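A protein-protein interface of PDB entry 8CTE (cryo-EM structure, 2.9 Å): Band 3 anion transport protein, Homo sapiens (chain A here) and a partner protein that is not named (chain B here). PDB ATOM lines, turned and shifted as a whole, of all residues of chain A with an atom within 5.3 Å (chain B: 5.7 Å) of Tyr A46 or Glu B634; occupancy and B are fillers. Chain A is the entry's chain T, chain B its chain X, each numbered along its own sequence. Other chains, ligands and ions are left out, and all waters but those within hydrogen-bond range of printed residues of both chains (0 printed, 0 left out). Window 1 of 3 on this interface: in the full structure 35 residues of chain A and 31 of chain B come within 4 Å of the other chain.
NH1 of Arg B253 lies within hydrogen-bond range of O of Asp A45, 3.3 Å away. The side-chain hydroxyl (OH) of Tyr A46 lies within hydrogen-bond range of the side-chain carboxylate (OE2) of Glu B634, 3.3 Å away. The guanidinium group (NH1) of Arg B253 lies within hydrogen-bond range of the backbone carbonyl oxygen (O) of His A47. The guanidinium group of Arg B633 is in salt-bridge range of the side-chain carboxylate of Asp A122, at 3.3 Å. The side-chain hydroxyl (OG1) of Thr A42 sits close to the side-chain carboxylate (OE2) of Glu B634 (2.3 Å).
The backbone carbonyl oxygen (O) of Ala A43 lies close to a ring nitrogen (NE2) of His A47 (3.1 Å). The guanidinium group of Arg B246 lies within salt-bridge range of the side-chain carboxylate of Glu B634. OE1 of Glu B667 is in salt-bridge range of NH2 of Arg B246 (2.8 Å).
Among the printed residues, pairs that only touch across the chains: Asp A45 with Pro B250 (3.3 Å), Tyr A46 with Arg B633 (3.5 Å), Asp A45 with Arg B246 (3.5 Å), Tyr A46 with Arg B246 (3.6 Å), Tyr A46 with Arg B253 (3.6 Å), Thr A48 with Arg B253 (3.6 Å) and Asp A122 with His B632 (3.7 Å).
Printed residues of chain B within 4 Å of Thr A42: Glu B634. Of chain B, only Arg B246, Arg B253, Arg B633 and Glu B634 come within 4 Å of Tyr A46. Printed residues of chain B within 4 Å of Thr A48: Arg B253. Of the printed residues of chain A, His B632 touches Asp A122. Of the printed residues of chain A, Arg B633 touches Tyr A46 and Asp A122. Of the printed residues of chain A, Glu B634 touches Thr A42 and Tyr A46. The nearest residue of chain B that does not touch Tyr A46 is Leu B626 (4.2 Å). The nearest printed residue of chain B that does not touch Thr A42 is Arg B246 (4.2 Å).
Hydrophobic or aromatic side chains of chain A that line the printed part of chain B: Tyr A46. Printed residues of chain B that touch a printed residue of chain A: Arg B246, Pro B250, Arg B253, His B632, Arg B633 and Glu B634. Along chain B the printed residues that touch a printed residue of chain A span positions 246 to 634. Among the printed residues, 12 pairs touch across the chains. Among the printed residues, Asp or Glu carboxylates within 4 Å of a Lys or Arg side-chain nitrogen of the other chain: Asp A122 with Arg B633 (2.4 Å).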
ATOM      1  N   THR A  42     -27.288  16.226  -6.124  1.00  0.00           N
ATOM      2  CA  THR A  42     -28.016  17.352  -6.690  1.00  0.00           C
ATOM      3  C   THR A  42     -27.127  18.567  -6.926  1.00  0.00           C
ATOM      4  O   THR A  42     -27.627  19.697  -6.928  1.00  0.00           O
ATOM      5  CB  THR A  42     -29.188  17.731  -5.784  1.00  0.00           C
ATOM      6  OG1 THR A  42     -28.713  17.954  -4.451  1.00  0.00           O
ATOM      7  CG2 THR A  42     -30.223  16.620  -5.771  1.00  0.00           C
ATOM      8  N   ALA A  43     -25.823  18.357  -7.123  1.00  0.00           N
ATOM      9  CA  ALA A  43     -24.915  19.468  -7.391  1.00  0.00           C
ATOM     10  C   ALA A  43     -25.243  20.142  -8.718  1.00  0.00           C
ATOM     11  O   ALA A  43     -25.163  21.370  -8.842  1.00  0.00           O
ATOM     12  CB  ALA A  43     -23.467  18.972  -7.382  1.00  0.00           C
ATOM     13  N   THR A  44     -25.614  19.348  -9.726  1.00  0.00           N
ATOM     14  CA  THR A  44     -25.930  19.885 -11.045  1.00  0.00           C
ATOM     15  C   THR A  44     -27.209  20.713 -11.062  1.00  0.00           C
ATOM     16  O   THR A  44     -27.431  21.454 -12.026  1.00  0.00           O
ATOM     17  CB  THR A  44     -26.043  18.750 -12.066  1.00  0.00           C
ATOM     18  OG1 THR A  44     -27.085  17.849 -11.672  1.00  0.00           O
ATOM     19  CG2 THR A  44     -24.730  17.989 -12.167  1.00  0.00           C
ATOM     20  N   ASP A  45     -28.053  20.609 -10.033  1.00  0.00           N
ATOM     21  CA  ASP A  45     -29.263  21.416  -9.971  1.00  0.00           C
ATOM     22  C   ASP A  45     -28.977  22.883  -9.678  1.00  0.00           C
ATOM     23  O   ASP A  45     -29.832  23.733  -9.950  1.00  0.00           O
ATOM     24  CB  ASP A  45     -30.218  20.859  -8.913  1.00  0.00           C
ATOM     25  CG  ASP A  45     -30.805  19.517  -9.303  1.00  0.00           C
ATOM     26  OD1 ASP A  45     -30.431  18.990 -10.372  1.00  0.00           O
ATOM     27  OD2 ASP A  45     -31.643  18.990  -8.542  1.00  0.00           O
ATOM     28  N   TYR A  46     -27.803  23.197  -9.133  1.00  0.00           N
ATOM     29  CA  TYR A  46     -27.426  24.565  -8.804  1.00  0.00           C
ATOM     30  C   TYR A  46     -26.458  25.160  -9.821  1.00  0.00           C
ATOM     31  O   TYR A  46     -25.885  26.227  -9.577  1.00  0.00           O
ATOM     32  CB  TYR A  46     -26.823  24.621  -7.400  1.00  0.00           C
ATOM     33  CG  TYR A  46     -27.740  24.091  -6.322  1.00  0.00           C
ATOM     34  CD1 TYR A  46     -28.702  24.906  -5.740  1.00  0.00           C
ATOM     35  CD2 TYR A  46     -27.645  22.776  -5.886  1.00  0.00           C
ATOM     36  CE1 TYR A  46     -29.544  24.427  -4.755  1.00  0.00           C
ATOM     37  CE2 TYR A  46     -28.483  22.287  -4.900  1.00  0.00           C
ATOM     38  CZ  TYR A  46     -29.430  23.117  -4.340  1.00  0.00           C
ATOM     39  OH  TYR A  46     -30.267  22.636  -3.359  1.00  0.00           O
ATOM     40  N   HIS A  47     -26.264  24.493 -10.955  1.00  0.00           N
ATOM     41  CA  HIS A  47     -25.355  24.966 -11.992  1.00  0.00           C
ATOM     42  C   HIS A  47     -26.109  25.893 -12.937  1.00  0.00           C
ATOM     43  O   HIS A  47     -27.030  25.459 -13.638  1.00  0.00           O
ATOM     44  CB  HIS A  47     -24.750  23.790 -12.757  1.00  0.00           C
ATOM     45  CG  HIS A  47     -23.832  22.940 -11.933  1.00  0.00           C
ATOM     46  ND1 HIS A  47     -23.313  21.749 -12.389  1.00  0.00           N
ATOM     47  CD2 HIS A  47     -23.337  23.112 -10.685  1.00  0.00           C
ATOM     48  CE1 HIS A  47     -22.540  21.221 -11.456  1.00  0.00           C
ATOM     49  NE2 HIS A  47     -22.538  22.029 -10.413  1.00  0.00           N
ATOM     50  N   THR A  48     -25.717  27.164 -12.956  1.00  0.00           N
ATOM     51  CA  THR A  48     -26.386  28.143 -13.799  1.00  0.00           C
ATOM     52  C   THR A  48     -25.996  27.959 -15.261  1.00  0.00           C
ATOM     53  O   THR A  48     -24.920  27.449 -15.585  1.00  0.00           O
ATOM     54  CB  THR A  48     -26.047  29.563 -13.344  1.00  0.00           C
ATOM     55  OG1 THR A  48     -26.657  30.512 -14.229  1.00  0.00           O
ATOM     56  CG2 THR A  48     -24.541  29.779 -13.335  1.00  0.00           C
ATOM     57  N   ASP A 122     -21.023  30.737  -7.310  1.00  0.00           N
ATOM     58  CA  ASP A 122     -22.281  31.453  -7.564  1.00  0.00           C
ATOM     59  C   ASP A 122     -23.067  31.695  -6.271  1.00  0.00           C
ATOM     60  O   ASP A 122     -24.226  31.307  -6.123  1.00  0.00           O
ATOM     61  CB  ASP A 122     -23.142  30.745  -8.623  1.00  0.00           C
ATOM     62  CG  ASP A 122     -23.447  29.293  -8.287  1.00  0.00           C
ATOM     63  OD1 ASP A 122     -22.566  28.431  -8.492  1.00  0.00           O
ATOM     64  OD2 ASP A 122     -24.574  29.013  -7.825  1.00  0.00           O
ATOM     65  N   ARG B 246     -35.640  19.884  -6.802  1.00  0.00           N
ATOM     66  CA  ARG B 246     -35.056  21.067  -6.184  1.00  0.00           C
ATOM     67  C   ARG B 246     -35.652  22.362  -6.727  1.00  0.00           C
ATOM     68  O   ARG B 246     -35.036  23.425  -6.598  1.00  0.00           O
ATOM     69  CB  ARG B 246     -33.537  21.064  -6.368  1.00  0.00           C
ATOM     70  CG  ARG B 246     -32.809  20.096  -5.452  1.00  0.00           C
ATOM     71  CD  ARG B 246     -33.015  20.470  -3.994  1.00  0.00           C
ATOM     72  NE  ARG B 246     -32.312  19.568  -3.090  1.00  0.00           N
ATOM     73  CZ  ARG B 246     -32.861  18.508  -2.512  1.00  0.00           C
ATOM     74  NH1 ARG B 246     -34.126  18.184  -2.722  1.00  0.00           N
ATOM     75  NH2 ARG B 246     -32.120  17.753  -1.707  1.00  0.00           N
ATOM     76  N   PRO B 250     -33.949  23.992 -12.009  1.00  0.00           N
ATOM     77  CA  PRO B 250     -33.215  22.866 -12.613  1.00  0.00           C
ATOM     78  C   PRO B 250     -34.010  22.129 -13.676  1.00  0.00           C
ATOM     79  O   PRO B 250     -33.426  21.661 -14.661  1.00  0.00           O
ATOM     80  CB  PRO B 250     -32.907  21.959 -11.413  1.00  0.00           C
ATOM     81  CG  PRO B 250     -32.985  22.850 -10.231  1.00  0.00           C
ATOM     82  CD  PRO B 250     -34.080  23.809 -10.550  1.00  0.00           C
ATOM     83  N   ARG B 253     -33.752  24.215 -16.783  1.00  0.00           N
ATOM     84  CA  ARG B 253     -32.406  24.095 -17.336  1.00  0.00           C
ATOM     85  C   ARG B 253     -32.222  22.768 -18.059  1.00  0.00           C
ATOM     86  O   ARG B 253     -31.636  22.722 -19.147  1.00  0.00           O
ATOM     87  CB  ARG B 253     -31.365  24.244 -16.226  1.00  0.00           C
ATOM     88  CG  ARG B 253     -31.263  25.639 -15.640  1.00  0.00           C
ATOM     89  CD  ARG B 253     -30.365  25.648 -14.413  1.00  0.00           C
ATOM     90  NE  ARG B 253     -30.273  26.968 -13.804  1.00  0.00           N
ATOM     91  CZ  ARG B 253     -29.681  27.218 -12.644  1.00  0.00           C
ATOM     92  NH1 ARG B 253     -29.122  26.253 -11.933  1.00  0.00           N
ATOM     93  NH2 ARG B 253     -29.651  28.466 -12.186  1.00  0.00           N
ATOM     94  N   SER B 624     -31.276  16.646   4.750  1.00  0.00           N
ATOM     95  CA  SER B 624     -30.766  17.784   4.000  1.00  0.00           C
ATOM     96  C   SER B 624     -31.576  19.028   4.335  1.00  0.00           C
ATOM     97  O   SER B 624     -32.794  18.955   4.527  1.00  0.00           O
ATOM     98  CB  SER B 624     -30.815  17.517   2.491  1.00  0.00           C
ATOM     99  OG  SER B 624     -30.060  16.368   2.150  1.00  0.00           O
ATOM    100  N   ILE B 625     -30.894  20.168   4.407  1.00  0.00           N
ATOM    101  CA  ILE B 625     -31.518  21.452   4.701  1.00  0.00           C
ATOM    102  C   ILE B 625     -31.177  22.422   3.580  1.00  0.00           C
ATOM    103  O   ILE B 625     -30.042  22.442   3.090  1.00  0.00           O
ATOM    104  CB  ILE B 625     -31.069  22.008   6.067  1.00  0.00           C
ATOM    105  CG1 ILE B 625     -29.543  21.976   6.192  1.00  0.00           C
ATOM    106  CG2 ILE B 625     -31.713  21.221   7.201  1.00  0.00           C
ATOM    107  CD1 ILE B 625     -29.023  22.557   7.487  1.00  0.00           C
ATOM    108  N   LEU B 626     -32.163  23.213   3.164  1.00  0.00           N
ATOM    109  CA  LEU B 626     -31.965  24.204   2.119  1.00  0.00           C
ATOM    110  C   LEU B 626     -32.959  25.342   2.304  1.00  0.00           C
ATOM    111  O   LEU B 626     -33.958  25.215   3.015  1.00  0.00           O
ATOM    112  CB  LEU B 626     -32.108  23.589   0.717  1.00  0.00           C
ATOM    113  CG  LEU B 626     -33.434  22.917   0.345  1.00  0.00           C
ATOM    114  CD1 LEU B 626     -34.345  23.858  -0.435  1.00  0.00           C
ATOM    115  CD2 LEU B 626     -33.183  21.640  -0.440  1.00  0.00           C
ATOM    116  N   ILE B 631     -29.502  29.381   3.385  1.00  0.00           N
ATOM    117  CA  ILE B 631     -28.415  28.434   3.184  1.00  0.00           C
ATOM    118  C   ILE B 631     -27.996  28.472   1.722  1.00  0.00           C
ATOM    119  O   ILE B 631     -28.834  28.434   0.815  1.00  0.00           O
ATOM    120  CB  ILE B 631     -28.823  26.999   3.594  1.00  0.00           C
ATOM    121  CG1 ILE B 631     -29.291  26.964   5.051  1.00  0.00           C
ATOM    122  CG2 ILE B 631     -27.674  26.025   3.378  1.00  0.00           C
ATOM    123  CD1 ILE B 631     -29.852  25.627   5.479  1.00  0.00           C
ATOM    124  N   HIS B 632     -26.687  28.560   1.495  1.00  0.00           N
ATOM    125  CA  HIS B 632     -26.147  28.496   0.143  1.00  0.00           C
ATOM    126  C   HIS B 632     -26.262  27.068  -0.373  1.00  0.00           C
ATOM    127  O   HIS B 632     -25.652  26.152   0.189  1.00  0.00           O
ATOM    128  CB  HIS B 632     -24.692  28.959   0.120  1.00  0.00           C
ATOM    129  CG  HIS B 632     -24.015  28.748  -1.199  1.00  0.00           C
ATOM    130  ND1 HIS B 632     -24.461  29.328  -2.366  1.00  0.00           N
ATOM    131  CD2 HIS B 632     -22.926  28.018  -1.533  1.00  0.00           C
ATOM    132  CE1 HIS B 632     -23.674  28.966  -3.363  1.00  0.00           C
ATOM    133  NE2 HIS B 632     -22.735  28.170  -2.885  1.00  0.00           N
ATOM    134  N   ARG B 633     -27.039  26.888  -1.439  1.00  0.00           N
ATOM    135  CA  ARG B 633     -27.350  25.575  -2.026  1.00  0.00           C
ATOM    136  C   ARG B 633     -27.966  24.722  -0.918  1.00  0.00           C
ATOM    137  O   ARG B 633     -28.907  25.184  -0.254  1.00  0.00           O
ATOM    138  CB  ARG B 633     -26.108  25.000  -2.697  1.00  0.00           C
ATOM    139  CG  ARG B 633     -25.579  25.850  -3.838  1.00  0.00           C
ATOM    140  CD  ARG B 633     -24.485  25.128  -4.599  1.00  0.00           C
ATOM    141  NE  ARG B 633     -24.045  25.878  -5.768  1.00  0.00           N
ATOM    142  CZ  ARG B 633     -23.217  25.407  -6.690  1.00  0.00           C
ATOM    143  NH1 ARG B 633     -22.725  24.182  -6.615  1.00  0.00           N
ATOM    144  NH2 ARG B 633     -22.876  26.186  -7.712  1.00  0.00           N
ATOM    145  N   GLU B 634     -27.491  23.504  -0.683  1.00  0.00           N
ATOM    146  CA  GLU B 634     -28.019  22.661   0.379  1.00  0.00           C
ATOM    147  C   GLU B 634     -26.880  21.944   1.086  1.00  0.00           C
ATOM    148  O   GLU B 634     -25.822  21.692   0.502  1.00  0.00           O
ATOM    149  CB  GLU B 634     -29.018  21.635  -0.166  1.00  0.00           C
ATOM    150  CG  GLU B 634     -28.461  20.777  -1.284  1.00  0.00           C
ATOM    151  CD  GLU B 634     -29.435  19.716  -1.743  1.00  0.00           C
ATOM    152  OE1 GLU B 634     -30.122  19.126  -0.885  1.00  0.00           O
ATOM    153  OE2 GLU B 634     -29.519  19.475  -2.965  1.00  0.00           O
ATOM    154  N   ARG B 635     -27.107  21.621   2.356  1.00  0.00           N
ATOM    155  CA  ARG B 635     -26.177  20.836   3.153  1.00  0.00           C
ATOM    156  C   ARG B 635     -26.859  19.540   3.562  1.00  0.00           C
ATOM    157  O   ARG B 635     -27.936  19.565   4.165  1.00  0.00           O
ATOM    158  CB  ARG B 635     -25.709  21.608   4.390  1.00  0.00           C
ATOM    159  CG  ARG B 635     -24.990  22.909   4.075  1.00  0.00           C
ATOM    160  CD  ARG B 635     -24.238  23.434   5.287  1.00  0.00           C
ATOM    161  NE  ARG B 635     -24.678  24.770   5.671  1.00  0.00           N
ATOM    162  CZ  ARG B 635     -25.499  25.029   6.679  1.00  0.00           C
ATOM    163  NH1 ARG B 635     -25.985  24.063   7.440  1.00  0.00           N
ATOM    164  NH2 ARG B 635     -25.838  26.290   6.930  1.00  0.00           N
ATOM    165  N   SER B 636     -26.231  18.415   3.237  1.00  0.00           N
ATOM    166  CA  SER B 636     -26.768  17.095   3.536  1.00  0.00           C
ATOM    167  C   SER B 636     -26.039  16.518   4.740  1.00  0.00           C
ATOM    168  O   SER B 636     -24.808  16.587   4.819  1.00  0.00           O
ATOM    169  CB  SER B 636     -26.633  16.160   2.330  1.00  0.00           C
ATOM    170  OG  SER B 636     -27.416  16.617   1.241  1.00  0.00           O
ATOM    171  N   GLU B 667     -35.393  17.944   4.149  1.00  0.00           N
ATOM    172  CA  GLU B 667     -35.700  16.695   3.469  1.00  0.00           C
ATOM    173  C   GLU B 667     -34.978  15.548   4.161  1.00  0.00           C
ATOM    174  O   GLU B 667     -33.790  15.653   4.480  1.00  0.00           O
ATOM    175  CB  GLU B 667     -35.297  16.758   1.993  1.00  0.00           C
ATOM    176  CG  GLU B 667     -35.664  15.522   1.193  1.00  0.00           C
ATOM    177  CD  GLU B 667     -35.212  15.609  -0.250  1.00  0.00           C
ATOM    178  OE1 GLU B 667     -34.153  16.219  -0.505  1.00  0.00           O
ATOM    179  OE2 GLU B 667     -35.919  15.075  -1.129  1.00  0.00           O
